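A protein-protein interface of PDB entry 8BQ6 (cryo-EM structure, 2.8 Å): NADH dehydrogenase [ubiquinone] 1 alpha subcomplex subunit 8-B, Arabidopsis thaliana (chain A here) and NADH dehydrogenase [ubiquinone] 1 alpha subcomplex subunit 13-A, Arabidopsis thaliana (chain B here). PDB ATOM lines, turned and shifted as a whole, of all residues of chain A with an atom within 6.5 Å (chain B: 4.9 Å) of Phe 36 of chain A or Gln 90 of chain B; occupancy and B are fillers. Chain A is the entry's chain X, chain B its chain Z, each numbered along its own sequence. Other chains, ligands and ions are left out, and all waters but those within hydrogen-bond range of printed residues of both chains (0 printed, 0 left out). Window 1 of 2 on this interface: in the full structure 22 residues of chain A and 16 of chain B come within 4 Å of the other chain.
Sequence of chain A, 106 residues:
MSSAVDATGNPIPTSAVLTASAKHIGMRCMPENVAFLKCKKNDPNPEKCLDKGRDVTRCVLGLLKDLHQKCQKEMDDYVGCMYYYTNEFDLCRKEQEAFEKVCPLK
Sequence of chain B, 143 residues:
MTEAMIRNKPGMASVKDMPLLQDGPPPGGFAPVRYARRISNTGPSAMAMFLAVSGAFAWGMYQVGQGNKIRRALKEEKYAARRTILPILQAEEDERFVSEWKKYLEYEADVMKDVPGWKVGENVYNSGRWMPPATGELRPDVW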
ATOM      1  N   PRO A  31     -15.658   7.418  19.538  1.00  0.00           N
ATOM      2  CA  PRO A  31     -14.810   8.486  20.100  1.00  0.00           C
ATOM      3  C   PRO A  31     -15.528   9.811  20.290  1.00  0.00           C
ATOM      4  O   PRO A  31     -15.347  10.461  21.329  1.00  0.00           O
ATOM      5  CB  PRO A  31     -13.667   8.605  19.079  1.00  0.00           C
ATOM      6  CG  PRO A  31     -13.732   7.371  18.254  1.00  0.00           C
ATOM      7  CD  PRO A  31     -15.169   6.992  18.215  1.00  0.00           C
ATOM      8  N   GLU A  32     -16.323  10.246  19.309  1.00  0.00           N
ATOM      9  CA  GLU A  32     -17.034  11.513  19.450  1.00  0.00           C
ATOM     10  C   GLU A  32     -18.050  11.449  20.584  1.00  0.00           C
ATOM     11  O   GLU A  32     -18.205  12.412  21.348  1.00  0.00           O
ATOM     12  CB  GLU A  32     -17.715  11.884  18.133  1.00  0.00           C
ATOM     13  CG  GLU A  32     -16.763  12.303  17.022  1.00  0.00           C
ATOM     14  CD  GLU A  32     -16.316  11.138  16.159  1.00  0.00           C
ATOM     15  OE1 GLU A  32     -16.747   9.998  16.426  1.00  0.00           O
ATOM     16  OE2 GLU A  32     -15.540  11.365  15.208  1.00  0.00           O
ATOM     17  N   ASN A  33     -18.745  10.315  20.710  1.00  0.00           N
ATOM     18  CA  ASN A  33     -19.658  10.109  21.830  1.00  0.00           C
ATOM     19  C   ASN A  33     -18.926  10.219  23.160  1.00  0.00           C
ATOM     20  O   ASN A  33     -19.403  10.874  24.093  1.00  0.00           O
ATOM     21  CB  ASN A  33     -20.329   8.738  21.716  1.00  0.00           C
ATOM     22  CG  ASN A  33     -21.490   8.722  20.739  1.00  0.00           C
ATOM     23  OD1 ASN A  33     -21.845   9.743  20.153  1.00  0.00           O
ATOM     24  ND2 ASN A  33     -22.088   7.552  20.563  1.00  0.00           N
ATOM     25  N   VAL A  34     -17.764   9.569  23.268  1.00  0.00           N
ATOM     26  CA  VAL A  34     -17.031   9.579  24.531  1.00  0.00           C
ATOM     27  C   VAL A  34     -16.564  10.988  24.868  1.00  0.00           C
ATOM     28  O   VAL A  34     -16.642  11.422  26.022  1.00  0.00           O
ATOM     29  CB  VAL A  34     -15.859   8.582  24.485  1.00  0.00           C
ATOM     30  CG1 VAL A  34     -14.940   8.779  25.684  1.00  0.00           C
ATOM     31  CG2 VAL A  34     -16.383   7.164  24.465  1.00  0.00           C
ATOM     32  N   ALA A  35     -16.073  11.725  23.868  1.00  0.00           N
ATOM     33  CA  ALA A  35     -15.612  13.091  24.112  1.00  0.00           C
ATOM     34  C   ALA A  35     -16.759  13.984  24.568  1.00  0.00           C
ATOM     35  O   ALA A  35     -16.621  14.765  25.523  1.00  0.00           O
ATOM     36  CB  ALA A  35     -14.964  13.655  22.849  1.00  0.00           C
ATOM     37  N   PHE A  36     -17.902  13.881  23.885  1.00  0.00           N
ATOM     38  CA  PHE A  36     -19.088  14.619  24.295  1.00  0.00           C
ATOM     39  C   PHE A  36     -19.470  14.300  25.732  1.00  0.00           C
ATOM     40  O   PHE A  36     -19.706  15.210  26.533  1.00  0.00           O
ATOM     41  CB  PHE A  36     -20.241  14.288  23.352  1.00  0.00           C
ATOM     42  CG  PHE A  36     -21.495  15.039  23.646  1.00  0.00           C
ATOM     43  CD1 PHE A  36     -21.655  16.337  23.211  1.00  0.00           C
ATOM     44  CD2 PHE A  36     -22.517  14.447  24.366  1.00  0.00           C
ATOM     45  CE1 PHE A  36     -22.812  17.026  23.479  1.00  0.00           C
ATOM     46  CE2 PHE A  36     -23.672  15.135  24.640  1.00  0.00           C
ATOM     47  CZ  PHE A  36     -23.819  16.428  24.197  1.00  0.00           C
ATOM     48  N   LEU A  37     -19.545  13.012  26.076  1.00  0.00           N
ATOM     49  CA  LEU A  37     -19.980  12.633  27.416  1.00  0.00           C
ATOM     50  C   LEU A  37     -18.984  13.094  28.473  1.00  0.00           C
ATOM     51  O   LEU A  37     -19.381  13.525  29.562  1.00  0.00           O
ATOM     52  CB  LEU A  37     -20.199  11.124  27.490  1.00  0.00           C
ATOM     53  CG  LEU A  37     -21.352  10.625  26.618  1.00  0.00           C
ATOM     54  CD1 LEU A  37     -21.517   9.120  26.722  1.00  0.00           C
ATOM     55  CD2 LEU A  37     -22.637  11.337  27.000  1.00  0.00           C
ATOM     56  N   LYS A  38     -17.688  13.025  28.168  1.00  0.00           N
ATOM     57  CA  LYS A  38     -16.679  13.490  29.111  1.00  0.00           C
ATOM     58  C   LYS A  38     -16.837  14.980  29.386  1.00  0.00           C
ATOM     59  O   LYS A  38     -16.844  15.419  30.545  1.00  0.00           O
ATOM     60  CB  LYS A  38     -15.284  13.184  28.568  1.00  0.00           C
ATOM     61  CG  LYS A  38     -14.189  13.276  29.606  1.00  0.00           C
ATOM     62  CD  LYS A  38     -13.365  12.000  29.662  1.00  0.00           C
ATOM     63  CE  LYS A  38     -13.161  11.389  28.282  1.00  0.00           C
ATOM     64  NZ  LYS A  38     -12.250  10.211  28.338  1.00  0.00           N
ATOM     65  N   CYS A  39     -16.993  15.775  28.328  1.00  0.00           N
ATOM     66  CA  CYS A  39     -17.108  17.211  28.548  1.00  0.00           C
ATOM     67  C   CYS A  39     -18.462  17.577  29.153  1.00  0.00           C
ATOM     68  O   CYS A  39     -18.576  18.589  29.854  1.00  0.00           O
ATOM     69  CB  CYS A  39     -16.836  17.956  27.244  1.00  0.00           C
ATOM     70  SG  CYS A  39     -17.845  17.459  25.882  1.00  0.00           S
ATOM     71  N   LYS A  40     -19.494  16.757  28.922  1.00  0.00           N
ATOM     72  CA  LYS A  40     -20.753  16.945  29.641  1.00  0.00           C
ATOM     73  C   LYS A  40     -20.568  16.691  31.130  1.00  0.00           C
ATOM     74  O   LYS A  40     -21.120  17.414  31.967  1.00  0.00           O
ATOM     75  CB  LYS A  40     -21.843  16.029  29.079  1.00  0.00           C
ATOM     76  CG  LYS A  40     -22.530  16.568  27.844  1.00  0.00           C
ATOM     77  CD  LYS A  40     -22.930  18.013  28.049  1.00  0.00           C
ATOM     78  CE  LYS A  40     -24.222  18.144  28.813  1.00  0.00           C
ATOM     79  NZ  LYS A  40     -25.046  19.246  28.255  1.00  0.00           N
ATOM     80  N   LYS A  41     -19.795  15.660  31.474  1.00  0.00           N
ATOM     81  CA  LYS A  41     -19.480  15.396  32.873  1.00  0.00           C
ATOM     82  C   LYS A  41     -18.755  16.574  33.508  1.00  0.00           C
ATOM     83  O   LYS A  41     -19.075  16.974  34.634  1.00  0.00           O
ATOM     84  CB  LYS A  41     -18.634  14.130  32.982  1.00  0.00           C
ATOM     85  CG  LYS A  41     -18.644  13.489  34.348  1.00  0.00           C
ATOM     86  CD  LYS A  41     -17.771  12.253  34.352  1.00  0.00           C
ATOM     87  CE  LYS A  41     -17.865  11.502  35.659  1.00  0.00           C
ATOM     88  NZ  LYS A  41     -16.717  10.575  35.854  1.00  0.00           N
ATOM     89  N   PRO A  46     -24.924  23.922  28.503  1.00  0.00           N
ATOM     90  CA  PRO A  46     -25.057  23.587  27.078  1.00  0.00           C
ATOM     91  C   PRO A  46     -24.172  24.413  26.158  1.00  0.00           C
ATOM     92  O   PRO A  46     -23.724  23.894  25.129  1.00  0.00           O
ATOM     93  CB  PRO A  46     -26.549  23.823  26.801  1.00  0.00           C
ATOM     94  CG  PRO A  46     -27.036  24.663  27.941  1.00  0.00           C
ATOM     95  CD  PRO A  46     -26.219  24.259  29.114  1.00  0.00           C
ATOM     96  N   CYS A  49     -20.375  23.205  25.261  1.00  0.00           N
ATOM     97  CA  CYS A  49     -20.110  21.878  24.615  1.00  0.00           C
ATOM     98  C   CYS A  49     -20.650  21.820  23.185  1.00  0.00           C
ATOM     99  O   CYS A  49     -20.650  20.715  22.615  1.00  0.00           O
ATOM    100  CB  CYS A  49     -20.765  20.709  25.346  1.00  0.00           C
ATOM    101  SG  CYS A  49     -20.142  20.390  27.016  1.00  0.00           S
ATOM    102  N   LEU A  50     -21.072  22.954  22.625  1.00  0.00           N
ATOM    103  CA  LEU A  50     -21.659  22.991  21.261  1.00  0.00           C
ATOM    104  C   LEU A  50     -20.671  22.430  20.228  1.00  0.00           C
ATOM    105  O   LEU A  50     -21.147  21.808  19.263  1.00  0.00           O
ATOM    106  CB  LEU A  50     -22.053  24.437  20.952  1.00  0.00           C
ATOM    107  CG  LEU A  50     -23.205  24.992  21.790  1.00  0.00           C
ATOM    108  CD1 LEU A  50     -23.510  26.429  21.408  1.00  0.00           C
ATOM    109  CD2 LEU A  50     -24.449  24.129  21.652  1.00  0.00           C
ATOM    110  N   LYS A  52     -18.092  19.953  20.709  1.00  0.00           N
ATOM    111  CA  LYS A  52     -18.088  18.473  20.842  1.00  0.00           C
ATOM    112  C   LYS A  52     -19.412  17.919  20.309  1.00  0.00           C
ATOM    113  O   LYS A  52     -19.391  16.831  19.723  1.00  0.00           O
ATOM    114  CB  LYS A  52     -17.849  18.066  22.299  1.00  0.00           C
ATOM    115  CG  LYS A  52     -16.439  17.588  22.608  1.00  0.00           C
ATOM    116  CD  LYS A  52     -15.460  18.730  22.769  1.00  0.00           C
ATOM    117  CE  LYS A  52     -14.093  18.287  23.240  1.00  0.00           C
ATOM    118  NZ  LYS A  52     -14.147  17.693  24.596  1.00  0.00           N
ATOM    119  N   GLY A  53     -20.504  18.654  20.503  1.00  0.00           N
ATOM    120  CA  GLY A  53     -21.818  18.233  19.988  1.00  0.00           C
ATOM    121  C   GLY A  53     -21.850  18.211  18.476  1.00  0.00           C
ATOM    122  O   GLY A  53     -22.433  17.266  17.925  1.00  0.00           O
ATOM    123  N   ARG A  54     -21.253  19.214  17.829  1.00  0.00           N
ATOM    124  CA  ARG A  54     -21.224  19.286  16.347  1.00  0.00           C
ATOM    125  C   ARG A  54     -20.427  18.105  15.787  1.00  0.00           C
ATOM    126  O   ARG A  54     -20.805  17.621  14.718  1.00  0.00           O
ATOM    127  CB  ARG A  54     -20.621  20.614  15.892  1.00  0.00           C
ATOM    128  CG  ARG A  54     -21.657  21.695  15.630  1.00  0.00           C
ATOM    129  CD  ARG A  54     -21.023  23.069  15.618  1.00  0.00           C
ATOM    130  NE  ARG A  54     -21.880  24.056  16.255  1.00  0.00           N
ATOM    131  CZ  ARG A  54     -21.475  24.929  17.169  1.00  0.00           C
ATOM    132  NH1 ARG A  54     -20.213  24.941  17.562  1.00  0.00           N
ATOM    133  NH2 ARG A  54     -22.335  25.789  17.684  1.00  0.00           N
ATOM    134  N   VAL A  56     -20.283  15.134  17.198  1.00  0.00           N
ATOM    135  CA  VAL A  56     -21.177  13.982  17.305  1.00  0.00           C
ATOM    136  C   VAL A  56     -22.210  14.010  16.186  1.00  0.00           C
ATOM    137  O   VAL A  56     -22.481  12.992  15.534  1.00  0.00           O
ATOM    138  CB  VAL A  56     -21.843  13.942  18.692  1.00  0.00           C
ATOM    139  CG1 VAL A  56     -23.166  13.198  18.632  1.00  0.00           C
ATOM    140  CG2 VAL A  56     -20.928  13.277  19.690  1.00  0.00           C
ATOM    141  N   LEU B  86     -27.690   8.606  22.716  1.00  0.00           N
ATOM    142  CA  LEU B  86     -27.805   9.671  23.708  1.00  0.00           C
ATOM    143  C   LEU B  86     -27.058  10.938  23.305  1.00  0.00           C
ATOM    144  O   LEU B  86     -27.655  12.029  23.378  1.00  0.00           O
ATOM    145  CB  LEU B  86     -27.329   9.124  25.060  1.00  0.00           C
ATOM    146  CG  LEU B  86     -27.415   9.954  26.336  1.00  0.00           C
ATOM    147  CD1 LEU B  86     -26.194  10.830  26.523  1.00  0.00           C
ATOM    148  CD2 LEU B  86     -28.638  10.783  26.274  1.00  0.00           C
ATOM    149  N   PRO B  87     -25.781  10.887  22.891  1.00  0.00           N
ATOM    150  CA  PRO B  87     -25.056  12.144  22.631  1.00  0.00           C
ATOM    151  C   PRO B  87     -25.674  13.031  21.566  1.00  0.00           C
ATOM    152  O   PRO B  87     -25.677  14.256  21.731  1.00  0.00           O
ATOM    153  CB  PRO B  87     -23.662  11.651  22.221  1.00  0.00           C
ATOM    154  CG  PRO B  87     -23.531  10.347  22.891  1.00  0.00           C
ATOM    155  CD  PRO B  87     -24.879   9.727  22.791  1.00  0.00           C
ATOM    156  N   ILE B  88     -26.201  12.465  20.480  1.00  0.00           N
ATOM    157  CA  ILE B  88     -26.758  13.319  19.435  1.00  0.00           C
ATOM    158  C   ILE B  88     -28.043  13.984  19.912  1.00  0.00           C
ATOM    159  O   ILE B  88     -28.291  15.161  19.623  1.00  0.00           O
ATOM    160  CB  ILE B  88     -26.961  12.527  18.129  1.00  0.00           C
ATOM    161  CG1 ILE B  88     -27.415  13.472  17.019  1.00  0.00           C
ATOM    162  CG2 ILE B  88     -27.948  11.394  18.313  1.00  0.00           C
ATOM    163  CD1 ILE B  88     -27.715  12.787  15.726  1.00  0.00           C
ATOM    164  N   LEU B  89     -28.874  13.252  20.659  1.00  0.00           N
ATOM    165  CA  LEU B  89     -30.086  13.853  21.202  1.00  0.00           C
ATOM    166  C   LEU B  89     -29.752  14.974  22.174  1.00  0.00           C
ATOM    167  O   LEU B  89     -30.382  16.041  22.147  1.00  0.00           O
ATOM    168  CB  LEU B  89     -30.941  12.791  21.888  1.00  0.00           C
ATOM    169  CG  LEU B  89     -31.356  11.614  21.013  1.00  0.00           C
ATOM    170  CD1 LEU B  89     -31.825  10.478  21.885  1.00  0.00           C
ATOM    171  CD2 LEU B  89     -32.441  12.032  20.035  1.00  0.00           C
ATOM    172  N   GLN B  90     -28.753  14.758  23.033  1.00  0.00           N
ATOM    173  CA  GLN B  90     -28.359  15.807  23.965  1.00  0.00           C
ATOM    174  C   GLN B  90     -27.787  17.014  23.233  1.00  0.00           C
ATOM    175  O   GLN B  90     -28.019  18.154  23.639  1.00  0.00           O
ATOM    176  CB  GLN B  90     -27.352  15.269  24.980  1.00  0.00           C
ATOM    177  CG  GLN B  90     -27.120  16.182  26.177  1.00  0.00           C
ATOM    178  CD  GLN B  90     -28.407  16.677  26.811  1.00  0.00           C
ATOM    179  OE1 GLN B  90     -29.102  15.930  27.493  1.00  0.00           O
ATOM    180  NE2 GLN B  90     -28.714  17.950  26.608  1.00  0.00           N
ATOM    181  N   ALA B  91     -27.028  16.786  22.157  1.00  0.00           N
ATOM    182  CA  ALA B  91     -26.462  17.906  21.409  1.00  0.00           C
ATOM    183  C   ALA B  91     -27.549  18.715  20.712  1.00  0.00           C
ATOM    184  O   ALA B  91     -27.503  19.954  20.693  1.00  0.00           O
ATOM    185  CB  ALA B  91     -25.439  17.395  20.395  1.00  0.00           C
ATOM    186  N   GLU B  92     -28.535  18.029  20.133  1.00  0.00           N
ATOM    187  CA  GLU B  92     -29.688  18.712  19.557  1.00  0.00           C
ATOM    188  C   GLU B  92     -30.402  19.554  20.608  1.00  0.00           C
ATOM    189  O   GLU B  92     -30.719  20.729  20.374  1.00  0.00           O
ATOM    190  CB  GLU B  92     -30.636  17.680  18.954  1.00  0.00           C
ATOM    191  CG  GLU B  92     -31.799  18.247  18.173  1.00  0.00           C
ATOM    192  CD  GLU B  92     -32.700  17.155  17.630  1.00  0.00           C
ATOM    193  OE1 GLU B  92     -32.382  16.599  16.559  1.00  0.00           O
ATOM    194  OE2 GLU B  92     -33.727  16.851  18.270  1.00  0.00           O
ATOM    195  N   GLU B  93     -30.650  18.968  21.782  1.00  0.00           N
ATOM    196  CA  GLU B  93     -31.337  19.705  22.837  1.00  0.00           C
ATOM    197  C   GLU B  93     -30.510  20.894  23.311  1.00  0.00           C
ATOM    198  O   GLU B  93     -31.059  21.952  23.634  1.00  0.00           O
ATOM    199  CB  GLU B  93     -31.668  18.767  24.000  1.00  0.00           C
ATOM    200  CG  GLU B  93     -32.059  19.456  25.305  1.00  0.00           C
ATOM    201  CD  GLU B  93     -33.419  20.138  25.259  1.00  0.00           C
ATOM    202  OE1 GLU B  93     -34.105  20.087  24.217  1.00  0.00           O
ATOM    203  OE2 GLU B  93     -33.806  20.733  26.285  1.00  0.00           O
ATOM    204  N   ASP B  94     -29.187  20.737  23.361  1.00  0.00           N
ATOM    205  CA  ASP B  94     -28.323  21.830  23.793  1.00  0.00           C
ATOM    206  C   ASP B  94     -28.379  22.990  22.811  1.00  0.00           C
ATOM    207  O   ASP B  94     -28.478  24.154  23.213  1.00  0.00           O
ATOM    208  CB  ASP B  94     -26.895  21.323  23.955  1.00  0.00           C
ATOM    209  CG  ASP B  94     -26.686  20.613  25.269  1.00  0.00           C
ATOM    210  OD1 ASP B  94     -27.634  20.596  26.076  1.00  0.00           O
ATOM    211  OD2 ASP B  94     -25.593  20.057  25.490  1.00  0.00           O
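The side-chain carboxylate (OD2) of Asp 94 of chain B lies within salt-bridge range of the side-chain amino group (NZ) of Lys 40 of chain A.
O of Phe 36 of chain A sits at hydrogen-bond distance from SG of Cys 39 of chain A, 3.0 Å away.
The side-chain carboxylate (OD1) of Asp 94 of chain B sits at hydrogen-bond distance from the side-chain amide nitrogen (NE2) of Gln 90 of chain B, at 2.9 Å.
Among the printed residues, pairs that only touch across the chains: Asn 33 of chain A with Pro 87 of chain B, Phe 36 of chain A with Pro 87 of chain B, Phe 36 of chain A with Gln 90 of chain B, Phe 36 of chain A with Ala 91 of chain B, Leu 37 of chain A with Leu 86 of chain B, Pro 46 of chain A with Asp 94 of chain B, Gly 53 of chain A with Ala 91 of chain B, Val 56 of chain A with Pro 87 of chain B and Val 56 of chain A with Ile 88 of chain B.
Gln 90 of chain B touches just one residue of chain A: Phe 36 (3.7 Å).
Of the printed residues of chain B, Lys 40 of chain A touches Asp 94 (2.9 Å).
Printed residues of chain A within 4 Å of Ala 91 of chain B: Phe 36 (3.8 Å) and Gly 53 (3.7 Å).
Printed residues of chain B within 4 Å of Leu 37 of chain A: Leu 86 (3.6 Å).
Printed residues of chain A within 4 Å of Pro 87 of chain B: Asn 33 (3.3 Å), Phe 36 (3.6 Å) and Val 56 (3.9 Å).
Cys 49 of chain A touches none of the printed residues of chain B.
Lys 41 of chain A touches none of the printed residues of chain B.
The nearest residue of chain A that does not touch Gln 90 of chain B is Lys 40 of chain A (4.2 Å).
Printed residues of chain A that touch a printed residue of chain B: Asn 33, Phe 36, Leu 37, Lys 40, Pro 46, Gly 53 and Val 56.
Along chain B the printed residues that touch a printed residue of chain A span positions 86 to 94.
Among the printed residues, 10 pairs touch across the chains.
Among the printed residues, Asp or Glu carboxylates within 4 Å of a Lys or Arg side-chain nitrogen of the other chain: Lys 40 of chain A with Asp 94 of chain B (2.9 Å).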
